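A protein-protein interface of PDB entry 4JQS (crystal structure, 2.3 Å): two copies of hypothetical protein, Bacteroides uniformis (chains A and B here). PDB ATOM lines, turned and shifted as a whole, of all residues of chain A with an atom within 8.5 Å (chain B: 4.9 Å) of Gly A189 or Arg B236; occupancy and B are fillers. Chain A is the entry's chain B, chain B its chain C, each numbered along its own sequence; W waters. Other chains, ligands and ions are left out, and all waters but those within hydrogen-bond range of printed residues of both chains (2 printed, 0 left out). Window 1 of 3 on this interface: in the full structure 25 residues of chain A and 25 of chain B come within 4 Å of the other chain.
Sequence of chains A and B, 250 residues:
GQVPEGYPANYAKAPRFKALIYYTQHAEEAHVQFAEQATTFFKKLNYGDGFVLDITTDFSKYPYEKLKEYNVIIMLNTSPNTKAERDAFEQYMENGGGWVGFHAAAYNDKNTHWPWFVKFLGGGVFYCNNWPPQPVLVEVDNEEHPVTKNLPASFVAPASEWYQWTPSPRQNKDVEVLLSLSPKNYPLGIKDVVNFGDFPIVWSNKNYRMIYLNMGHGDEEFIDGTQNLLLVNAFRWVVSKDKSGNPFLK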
ATOM      1  N   ASN A 129       3.365  19.529  -0.816  1.00  0.00           N
ATOM      2  CA  ASN A 129       3.209  19.548   0.623  1.00  0.00           C
ATOM      3  C   ASN A 129       1.790  19.942   0.993  1.00  0.00           C
ATOM      4  O   ASN A 129       1.073  20.545   0.177  1.00  0.00           O
ATOM      5  CB  ASN A 129       4.212  20.542   1.256  1.00  0.00           C
ATOM      6  CG  ASN A 129       3.931  21.979   0.866  1.00  0.00           C
ATOM      7  OD1 ASN A 129       4.263  22.414  -0.239  1.00  0.00           O
ATOM      8  ND2 ASN A 129       3.243  22.727   1.730  1.00  0.00           N
ATOM      9  N   ASN A 130       1.405  19.636   2.232  1.00  0.00           N
ATOM     10  CA  ASN A 130       0.129  20.086   2.782  1.00  0.00           C
ATOM     11  C   ASN A 130       0.389  21.390   3.526  1.00  0.00           C
ATOM     12  O   ASN A 130       1.535  21.696   3.869  1.00  0.00           O
ATOM     13  CB  ASN A 130      -0.463  19.033   3.745  1.00  0.00           C
ATOM     14  CG  ASN A 130       0.347  18.873   5.008  1.00  0.00           C
ATOM     15  OD1 ASN A 130       1.543  18.559   4.976  1.00  0.00           O
ATOM     16  ND2 ASN A 130      -0.256  19.195   6.137  1.00  0.00           N
ATOM     17  N   TRP A 131      -0.680  22.131   3.806  1.00  0.00           N
ATOM     18  CA  TRP A 131      -0.638  23.337   4.618  1.00  0.00           C
ATOM     19  C   TRP A 131      -2.023  23.528   5.246  1.00  0.00           C
ATOM     20  O   TRP A 131      -3.013  23.281   4.561  1.00  0.00           O
ATOM     21  CB  TRP A 131      -0.169  24.576   3.832  1.00  0.00           C
ATOM     22  CG  TRP A 131       0.265  25.677   4.750  1.00  0.00           C
ATOM     23  CD1 TRP A 131      -0.490  26.733   5.173  1.00  0.00           C
ATOM     24  CD2 TRP A 131       1.492  25.728   5.504  1.00  0.00           C
ATOM     25  NE1 TRP A 131       0.212  27.474   6.096  1.00  0.00           N
ATOM     26  CE2 TRP A 131       1.428  26.879   6.325  1.00  0.00           C
ATOM     27  CE3 TRP A 131       2.663  24.935   5.526  1.00  0.00           C
ATOM     28  CZ2 TRP A 131       2.500  27.275   7.157  1.00  0.00           C
ATOM     29  CZ3 TRP A 131       3.726  25.323   6.343  1.00  0.00           C
ATOM     30  CH2 TRP A 131       3.646  26.483   7.144  1.00  0.00           C
ATOM     31  N   PRO A 132      -2.140  23.885   6.548  1.00  0.00           N
ATOM     32  CA  PRO A 132      -1.075  24.229   7.507  1.00  0.00           C
ATOM     33  C   PRO A 132      -0.457  22.996   8.158  1.00  0.00           C
ATOM     34  O   PRO A 132      -1.017  21.903   8.005  1.00  0.00           O
ATOM     35  CB  PRO A 132      -1.833  25.075   8.547  1.00  0.00           C
ATOM     36  CG  PRO A 132      -3.187  24.422   8.582  1.00  0.00           C
ATOM     37  CD  PRO A 132      -3.478  24.086   7.152  1.00  0.00           C
ATOM     38  N   PRO A 133       0.649  23.140   8.934  1.00  0.00           N
ATOM     39  CA  PRO A 133       1.152  21.986   9.700  1.00  0.00           C
ATOM     40  C   PRO A 133       0.043  21.351  10.566  1.00  0.00           C
ATOM     41  O   PRO A 133      -0.777  22.060  11.172  1.00  0.00           O
ATOM     42  CB  PRO A 133       2.246  22.605  10.582  1.00  0.00           C
ATOM     43  CG  PRO A 133       2.677  23.814   9.827  1.00  0.00           C
ATOM     44  CD  PRO A 133       1.432  24.356   9.234  1.00  0.00           C
ATOM     45  N   GLN A 134      -0.018  20.023  10.591  1.00  0.00           N
ATOM     46  CA  GLN A 134      -1.034  19.363  11.398  1.00  0.00           C
ATOM     47  C   GLN A 134      -0.584  17.974  11.812  1.00  0.00           C
ATOM     48  O   GLN A 134       0.284  17.399  11.154  1.00  0.00           O
ATOM     49  CB  GLN A 134      -2.372  19.281  10.631  1.00  0.00           C
ATOM     50  CG  GLN A 134      -2.331  18.400   9.375  1.00  0.00           C
ATOM     51  CD  GLN A 134      -3.724  17.979   9.025  1.00  0.00           C
ATOM     52  OE1 GLN A 134      -4.437  18.656   8.270  1.00  0.00           O
ATOM     53  NE2 GLN A 134      -4.136  16.838   9.555  1.00  0.00           N
ATOM     54  N   PRO A 135      -1.178  17.389  12.888  1.00  0.00           N
ATOM     55  CA  PRO A 135      -0.853  15.988  13.209  1.00  0.00           C
ATOM     56  C   PRO A 135      -1.380  15.065  12.108  1.00  0.00           C
ATOM     57  O   PRO A 135      -2.311  15.439  11.394  1.00  0.00           O
ATOM     58  CB  PRO A 135      -1.593  15.741  14.534  1.00  0.00           C
ATOM     59  CG  PRO A 135      -2.137  17.060  14.971  1.00  0.00           C
ATOM     60  CD  PRO A 135      -2.256  17.904  13.765  1.00  0.00           C
ATOM     61  N   VAL A 136      -0.783  13.880  11.948  1.00  0.00           N
ATOM     62  CA  VAL A 136      -1.206  12.894  10.952  1.00  0.00           C
ATOM     63  C   VAL A 136      -1.027  11.479  11.503  1.00  0.00           C
ATOM     64  O   VAL A 136      -0.143  11.234  12.328  1.00  0.00           O
ATOM     65  CB  VAL A 136      -0.460  13.013   9.573  1.00  0.00           C
ATOM     66  CG1 VAL A 136      -0.892  14.234   8.776  1.00  0.00           C
ATOM     67  CG2 VAL A 136       1.059  12.955   9.730  1.00  0.00           C
ATOM     68  N   TRP A 162       4.233  18.383   5.834  1.00  0.00           N
ATOM     69  CA  TRP A 162       4.706  17.104   5.294  1.00  0.00           C
ATOM     70  C   TRP A 162       4.980  17.226   3.799  1.00  0.00           C
ATOM     71  O   TRP A 162       4.231  17.910   3.120  1.00  0.00           O
ATOM     72  CB  TRP A 162       3.694  15.981   5.606  1.00  0.00           C
ATOM     73  CG  TRP A 162       3.350  15.872   7.064  1.00  0.00           C
ATOM     74  CD1 TRP A 162       2.281  16.437   7.698  1.00  0.00           C
ATOM     75  CD2 TRP A 162       4.140  15.240   8.091  1.00  0.00           C
ATOM     76  NE1 TRP A 162       2.334  16.167   9.049  1.00  0.00           N
ATOM     77  CE2 TRP A 162       3.464  15.432   9.317  1.00  0.00           C
ATOM     78  CE3 TRP A 162       5.341  14.502   8.088  1.00  0.00           C
ATOM     79  CZ2 TRP A 162       3.935  14.893  10.524  1.00  0.00           C
ATOM     80  CZ3 TRP A 162       5.803  13.972   9.285  1.00  0.00           C
ATOM     81  CH2 TRP A 162       5.108  14.177  10.484  1.00  0.00           C
ATOM     82  N   ASN A 185      -5.275   9.678   5.864  1.00  0.00           N
ATOM     83  CA  ASN A 185      -5.224  11.120   6.134  1.00  0.00           C
ATOM     84  C   ASN A 185      -5.776  11.923   4.970  1.00  0.00           C
ATOM     85  O   ASN A 185      -6.091  13.100   5.160  1.00  0.00           O
ATOM     86  CB  ASN A 185      -3.777  11.558   6.403  1.00  0.00           C
ATOM     87  CG  ASN A 185      -3.222  11.043   7.698  1.00  0.00           C
ATOM     88  OD1 ASN A 185      -3.728  11.349   8.783  1.00  0.00           O
ATOM     89  ND2 ASN A 185      -2.147  10.281   7.615  1.00  0.00           N
ATOM     90  N   TYR A 186      -5.847  11.307   3.753  1.00  0.00           N
ATOM     91  CA  TYR A 186      -6.323  11.959   2.532  1.00  0.00           C
ATOM     92  C   TYR A 186      -7.824  12.204   2.536  1.00  0.00           C
ATOM     93  O   TYR A 186      -8.572  11.290   2.890  1.00  0.00           O
ATOM     94  CB  TYR A 186      -5.961  11.141   1.279  1.00  0.00           C
ATOM     95  CG  TYR A 186      -4.481  11.064   0.968  1.00  0.00           C
ATOM     96  CD1 TYR A 186      -3.651  12.166   1.153  1.00  0.00           C
ATOM     97  CD2 TYR A 186      -3.930   9.920   0.397  1.00  0.00           C
ATOM     98  CE1 TYR A 186      -2.305  12.121   0.804  1.00  0.00           C
ATOM     99  CE2 TYR A 186      -2.581   9.854   0.073  1.00  0.00           C
ATOM    100  CZ  TYR A 186      -1.774  10.963   0.263  1.00  0.00           C
ATOM    101  OH  TYR A 186      -0.449  10.924  -0.084  1.00  0.00           O
ATOM    102  N   PRO A 187      -8.306  13.383   2.060  1.00  0.00           N
ATOM    103  CA  PRO A 187      -7.537  14.555   1.597  1.00  0.00           C
ATOM    104  C   PRO A 187      -6.928  15.304   2.786  1.00  0.00           C
ATOM    105  O   PRO A 187      -7.598  15.544   3.800  1.00  0.00           O
ATOM    106  CB  PRO A 187      -8.561  15.364   0.799  1.00  0.00           C
ATOM    107  CG  PRO A 187      -9.905  14.962   1.330  1.00  0.00           C
ATOM    108  CD  PRO A 187      -9.765  13.606   1.968  1.00  0.00           C
ATOM    109  N   LEU A 188      -5.619  15.592   2.678  1.00  0.00           N
ATOM    110  CA  LEU A 188      -4.818  16.210   3.722  1.00  0.00           C
ATOM    111  C   LEU A 188      -4.490  17.668   3.421  1.00  0.00           C
ATOM    112  O   LEU A 188      -3.711  17.947   2.504  1.00  0.00           O
ATOM    113  CB  LEU A 188      -3.499  15.395   3.913  1.00  0.00           C
ATOM    114  CG  LEU A 188      -2.478  15.941   4.931  1.00  0.00           C
ATOM    115  CD1 LEU A 188      -3.045  15.943   6.324  1.00  0.00           C
ATOM    116  CD2 LEU A 188      -1.187  15.153   4.886  1.00  0.00           C
ATOM    117  N   GLY A 189      -5.025  18.560   4.244  1.00  0.00           N
ATOM    118  CA  GLY A 189      -4.784  19.994   4.150  1.00  0.00           C
ATOM    119  C   GLY A 189      -6.016  20.864   4.265  1.00  0.00           C
ATOM    120  O   GLY A 189      -7.122  20.441   3.901  1.00  0.00           O
ATOM    121  N   ILE A 190      -5.820  22.096   4.795  1.00  0.00           N
ATOM    122  CA  ILE A 190      -6.860  23.121   4.935  1.00  0.00           C
ATOM    123  C   ILE A 190      -6.585  24.165   3.843  1.00  0.00           C
ATOM    124  O   ILE A 190      -7.470  24.452   3.058  1.00  0.00           O
ATOM    125  CB  ILE A 190      -6.982  23.762   6.362  1.00  0.00           C
ATOM    126  CG1 ILE A 190      -7.009  22.737   7.537  1.00  0.00           C
ATOM    127  CG2 ILE A 190      -8.111  24.805   6.446  1.00  0.00           C
ATOM    128  CD1 ILE A 190      -8.132  21.725   7.575  1.00  0.00           C
ATOM    129  N   LYS A 191      -5.352  24.699   3.769  1.00  0.00           N
ATOM    130  CA  LYS A 191      -4.987  25.653   2.722  1.00  0.00           C
ATOM    131  C   LYS A 191      -4.564  24.907   1.452  1.00  0.00           C
ATOM    132  O   LYS A 191      -5.205  25.047   0.407  1.00  0.00           O
ATOM    133  CB  LYS A 191      -3.875  26.609   3.181  1.00  0.00           C
ATOM    134  CG  LYS A 191      -3.603  27.679   2.135  1.00  0.00           C
ATOM    135  CD  LYS A 191      -2.412  28.522   2.467  1.00  0.00           C
ATOM    136  CE  LYS A 191      -2.235  29.602   1.426  1.00  0.00           C
ATOM    137  NZ  LYS A 191      -0.981  30.360   1.671  1.00  0.00           N
ATOM    138  N   ASP A 192      -3.489  24.126   1.555  1.00  0.00           N
ATOM    139  CA  ASP A 192      -2.889  23.352   0.466  1.00  0.00           C
ATOM    140  C   ASP A 192      -3.167  21.880   0.748  1.00  0.00           C
ATOM    141  O   ASP A 192      -2.734  21.344   1.769  1.00  0.00           O
ATOM    142  CB  ASP A 192      -1.387  23.695   0.338  1.00  0.00           C
ATOM    143  CG  ASP A 192      -1.157  25.199   0.240  1.00  0.00           C
ATOM    144  OD1 ASP A 192      -2.008  25.898  -0.366  1.00  0.00           O
ATOM    145  OD2 ASP A 192      -0.151  25.676   0.770  1.00  0.00           O
ATOM    146  N   VAL A 193      -4.003  21.278  -0.112  1.00  0.00           N
ATOM    147  CA  VAL A 193      -4.557  19.932   0.023  1.00  0.00           C
ATOM    148  C   VAL A 193      -3.836  18.914  -0.872  1.00  0.00           C
ATOM    149  O   VAL A 193      -3.769  19.096  -2.086  1.00  0.00           O
ATOM    150  CB  VAL A 193      -6.088  19.958  -0.298  1.00  0.00           C
ATOM    151  CG1 VAL A 193      -6.750  18.616   0.003  1.00  0.00           C
ATOM    152  CG2 VAL A 193      -6.799  21.090   0.454  1.00  0.00           C
ATOM    153  N   VAL A 194      -3.329  17.829  -0.254  1.00  0.00           N
ATOM    154  CA  VAL A 194      -2.706  16.678  -0.935  1.00  0.00           C
ATOM    155  C   VAL A 194      -3.814  15.605  -0.954  1.00  0.00           C
ATOM    156  O   VAL A 194      -4.368  15.260   0.096  1.00  0.00           O
ATOM    157  CB  VAL A 194      -1.374  16.212  -0.280  1.00  0.00           C
ATOM    158  CG1 VAL A 194      -0.743  15.072  -1.074  1.00  0.00           C
ATOM    159  CG2 VAL A 194      -0.391  17.375  -0.138  1.00  0.00           C
ATOM    160  N   ASN A 195      -4.188  15.161  -2.157  1.00  0.00           N
ATOM    161  CA  ASN A 195      -5.305  14.259  -2.403  1.00  0.00           C
ATOM    162  C   ASN A 195      -4.938  12.785  -2.601  1.00  0.00           C
ATOM    163  O   ASN A 195      -5.812  11.935  -2.428  1.00  0.00           O
ATOM    164  CB  ASN A 195      -6.085  14.755  -3.628  1.00  0.00           C
ATOM    165  CG  ASN A 195      -6.737  16.106  -3.381  1.00  0.00           C
ATOM    166  OD1 ASN A 195      -7.565  16.271  -2.467  1.00  0.00           O
ATOM    167  ND2 ASN A 195      -6.322  17.121  -4.141  1.00  0.00           N
ATOM    168  N   VAL B 232      -8.820  19.074  14.259  1.00  0.00           N
ATOM    169  CA  VAL B 232      -8.571  19.464  12.863  1.00  0.00           C
ATOM    170  C   VAL B 232      -9.664  18.799  11.991  1.00  0.00           C
ATOM    171  O   VAL B 232     -10.320  19.466  11.190  1.00  0.00           O
ATOM    172  CB  VAL B 232      -7.138  19.083  12.406  1.00  0.00           C
ATOM    173  CG1 VAL B 232      -6.978  19.202  10.884  1.00  0.00           C
ATOM    174  CG2 VAL B 232      -6.078  19.913  13.137  1.00  0.00           C
ATOM    175  N   ASN B 233      -9.883  17.496  12.211  1.00  0.00           N
ATOM    176  CA  ASN B 233     -10.858  16.665  11.496  1.00  0.00           C
ATOM    177  C   ASN B 233     -12.283  17.168  11.657  1.00  0.00           C
ATOM    178  O   ASN B 233     -12.997  17.229  10.665  1.00  0.00           O
ATOM    179  CB  ASN B 233     -10.764  15.218  11.965  1.00  0.00           C
ATOM    180  CG  ASN B 233      -9.515  14.490  11.518  1.00  0.00           C
ATOM    181  OD1 ASN B 233      -8.664  15.027  10.803  1.00  0.00           O
ATOM    182  ND2 ASN B 233      -9.393  13.235  11.916  1.00  0.00           N
ATOM    183  N   ALA B 234     -12.683  17.540  12.895  1.00  0.00           N
ATOM    184  CA  ALA B 234     -14.014  18.049  13.255  1.00  0.00           C
ATOM    185  C   ALA B 234     -14.322  19.335  12.491  1.00  0.00           C
ATOM    186  O   ALA B 234     -15.370  19.425  11.851  1.00  0.00           O
ATOM    187  CB  ALA B 234     -14.078  18.299  14.760  1.00  0.00           C
ATOM    188  N   PHE B 235     -13.377  20.311  12.542  1.00  0.00           N
ATOM    189  CA  PHE B 235     -13.437  21.617  11.888  1.00  0.00           C
ATOM    190  C   PHE B 235     -13.496  21.452  10.363  1.00  0.00           C
ATOM    191  O   PHE B 235     -14.380  22.029   9.718  1.00  0.00           O
ATOM    192  CB  PHE B 235     -12.206  22.460  12.310  1.00  0.00           C
ATOM    193  CG  PHE B 235     -11.961  23.760  11.564  1.00  0.00           C
ATOM    194  CD1 PHE B 235     -12.888  24.798  11.612  1.00  0.00           C
ATOM    195  CD2 PHE B 235     -10.772  23.973  10.877  1.00  0.00           C
ATOM    196  CE1 PHE B 235     -12.647  26.009  10.963  1.00  0.00           C
ATOM    197  CE2 PHE B 235     -10.543  25.179  10.201  1.00  0.00           C
ATOM    198  CZ  PHE B 235     -11.481  26.193  10.259  1.00  0.00           C
ATOM    199  N   ARG B 236     -12.581  20.641   9.800  1.00  0.00           N
ATOM    200  CA  ARG B 236     -12.493  20.376   8.361  1.00  0.00           C
ATOM    201  C   ARG B 236     -13.787  19.752   7.804  1.00  0.00           C
ATOM    202  O   ARG B 236     -14.239  20.151   6.732  1.00  0.00           O
ATOM    203  CB  ARG B 236     -11.290  19.457   8.061  1.00  0.00           C
ATOM    204  CG  ARG B 236     -10.918  19.408   6.600  1.00  0.00           C
ATOM    205  CD  ARG B 236      -9.869  18.346   6.290  1.00  0.00           C
ATOM    206  NE  ARG B 236      -9.205  18.639   5.014  1.00  0.00           N
ATOM    207  CZ  ARG B 236      -9.733  18.444   3.806  1.00  0.00           C
ATOM    208  NH1 ARG B 236     -10.944  17.910   3.680  1.00  0.00           N
ATOM    209  NH2 ARG B 236      -9.065  18.799   2.718  1.00  0.00           N
ATOM    210  N   TRP B 237     -14.374  18.792   8.523  1.00  0.00           N
ATOM    211  CA  TRP B 237     -15.579  18.086   8.067  1.00  0.00           C
ATOM    212  C   TRP B 237     -16.789  19.034   7.980  1.00  0.00           C
ATOM    213  O   TRP B 237     -17.465  19.034   6.951  1.00  0.00           O
ATOM    214  CB  TRP B 237     -15.884  16.880   8.970  1.00  0.00           C
ATOM    215  CG  TRP B 237     -17.144  16.136   8.596  1.00  0.00           C
ATOM    216  CD1 TRP B 237     -17.377  15.426   7.452  1.00  0.00           C
ATOM    217  CD2 TRP B 237     -18.346  16.043   9.379  1.00  0.00           C
ATOM    218  NE1 TRP B 237     -18.649  14.899   7.473  1.00  0.00           N
ATOM    219  CE2 TRP B 237     -19.268  15.270   8.640  1.00  0.00           C
ATOM    220  CE3 TRP B 237     -18.722  16.525  10.649  1.00  0.00           C
ATOM    221  CZ2 TRP B 237     -20.543  14.954   9.132  1.00  0.00           C
ATOM    222  CZ3 TRP B 237     -19.973  16.200  11.138  1.00  0.00           C
ATOM    223  CH2 TRP B 237     -20.872  15.434  10.385  1.00  0.00           C
ATOM    224  N   VAL B 238     -17.039  19.849   9.030  1.00  0.00           N
ATOM    225  CA  VAL B 238     -18.149  20.809   9.048  1.00  0.00           C
ATOM    226  C   VAL B 238     -17.968  21.854   7.896  1.00  0.00           C
ATOM    227  O   VAL B 238     -18.934  22.173   7.202  1.00  0.00           O
ATOM    228  CB  VAL B 238     -18.298  21.476  10.452  1.00  0.00           C
ATOM    229  CG1 VAL B 238     -19.092  22.786  10.401  1.00  0.00           C
ATOM    230  CG2 VAL B 238     -18.931  20.510  11.442  1.00  0.00           C
ATOM    231  N   VAL B 239     -16.733  22.349   7.689  1.00  0.00           N
ATOM    232  CA  VAL B 239     -16.431  23.332   6.653  1.00  0.00           C
ATOM    233  C   VAL B 239     -16.681  22.745   5.250  1.00  0.00           C
ATOM    234  O   VAL B 239     -17.289  23.412   4.397  1.00  0.00           O
ATOM    235  CB  VAL B 239     -14.983  23.868   6.806  1.00  0.00           C
ATOM    236  CG1 VAL B 239     -14.516  24.628   5.561  1.00  0.00           C
ATOM    237  CG2 VAL B 239     -14.854  24.736   8.043  1.00  0.00           C
ATOM    238  N   SER B 240     -16.230  21.491   5.035  1.00  0.00           N
ATOM    239  CA  SER B 240     -16.319  20.805   3.748  1.00  0.00           C
ATOM    240  C   SER B 240     -17.752  20.513   3.314  1.00  0.00           C
ATOM    241  O   SER B 240     -17.953  20.314   2.123  1.00  0.00           O
ATOM    242  CB  SER B 240     -15.533  19.498   3.780  1.00  0.00           C
ATOM    243  OG  SER B 240     -16.243  18.475   4.460  1.00  0.00           O
ATOM    244  N   PHE B 248     -12.618  23.123  -0.105  1.00  0.00           N
ATOM    245  CA  PHE B 248     -11.318  22.495  -0.339  1.00  0.00           C
ATOM    246  C   PHE B 248     -11.139  21.989  -1.777  1.00  0.00           C
ATOM    247  O   PHE B 248     -10.051  21.532  -2.105  1.00  0.00           O
ATOM    248  CB  PHE B 248     -11.091  21.364   0.674  1.00  0.00           C
ATOM    249  CG  PHE B 248     -11.211  21.865   2.094  1.00  0.00           C
ATOM    250  CD1 PHE B 248     -10.312  22.805   2.596  1.00  0.00           C
ATOM    251  CD2 PHE B 248     -12.236  21.418   2.924  1.00  0.00           C
ATOM    252  CE1 PHE B 248     -10.442  23.295   3.891  1.00  0.00           C
ATOM    253  CE2 PHE B 248     -12.347  21.884   4.229  1.00  0.00           C
ATOM    254  CZ  PHE B 248     -11.438  22.810   4.710  1.00  0.00           C
HETATM  255  O   HOH W   1      -6.499  18.143   6.759  1.00  0.00           O
HETATM  256  O   HOH W   2      -6.856  15.142   8.584  1.00  0.00           O
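No position is printed for both chains.
Of the 6 pairs that touch across the chains among the printed residues, none has its exchanged pair printed and touching as well.
N of Ile A190 sits at hydrogen-bond distance from O of Trp A131 (3.1 Å).
NE1 of Trp A162 lies within hydrogen-bond range of O of Gln A134 (3.2 Å).
OG of Ser B240 sits close to O of Arg B236 (3.5 Å).
Of the 10 printed residues of chain B, 3 touch a printed residue of chain A.
Hydrophobic or aromatic side chains of chain B within 4 Å of the printed part of chain A: Val B232 and Phe B248.
Of the 20 printed residues of chain A, 5 touch a printed residue of chain B.
Among the printed residues, 6 pairs touch across the chains.
Gly A189 touches one residue of chain B.
Arg B236 touches just these residues of chain A: Pro A187 (3.6 Å), Gly A189 (2.8 Å), Ile A190 (3.8 Å) and Val A193 (3.6 Å).
Printed residues of chain A within 4 Å of Phe B248: Ile A190 (3.3 Å).
Printed residues of chain B within 4 Å of Ile A190: Arg B236 (3.8 Å) and Phe B248 (3.3 Å).
Of the printed residues of chain B, Pro A187 touches Arg B236 (3.6 Å).
Of the printed residues of chain B, Gln A134 touches Val B232 (3.7 Å).
Of the printed residues of chain B, Val A193 touches Arg B236.
Leu A188 touches none of the printed residues of chain B.
Val A194 touches none of the printed residues of chain B.
The nearest residue of chain A that does not touch Arg B236 is Leu A188 (4.7 Å).
The nearest printed residue of chain B that does not touch Ile A190 is Val B232 (4.3 Å).
Water W1 lies within hydrogen-bond range of OE1 of Gln A134 (2.6 Å), N of Gly A189 (2.9 Å) and NE of Arg B236 (3.3 Å).
Water W2 lies within hydrogen-bond range of OD1 of Asn B233 (2.9 Å) and NE2 of Gln A134 (3.3 Å).
NH2 of Arg B236 lies within hydrogen-bond range of O of Gly A189 (2.8 Å).
Val B232 touches Gln A134.
CZ of Arg B236 touches O of Pro A187, 3.6 Å away.
CG of Arg B236 touches CD1 of Ile A190, at 3.8 Å.
Ile A190 touches Phe B248.
Val A193 touches Arg B236.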
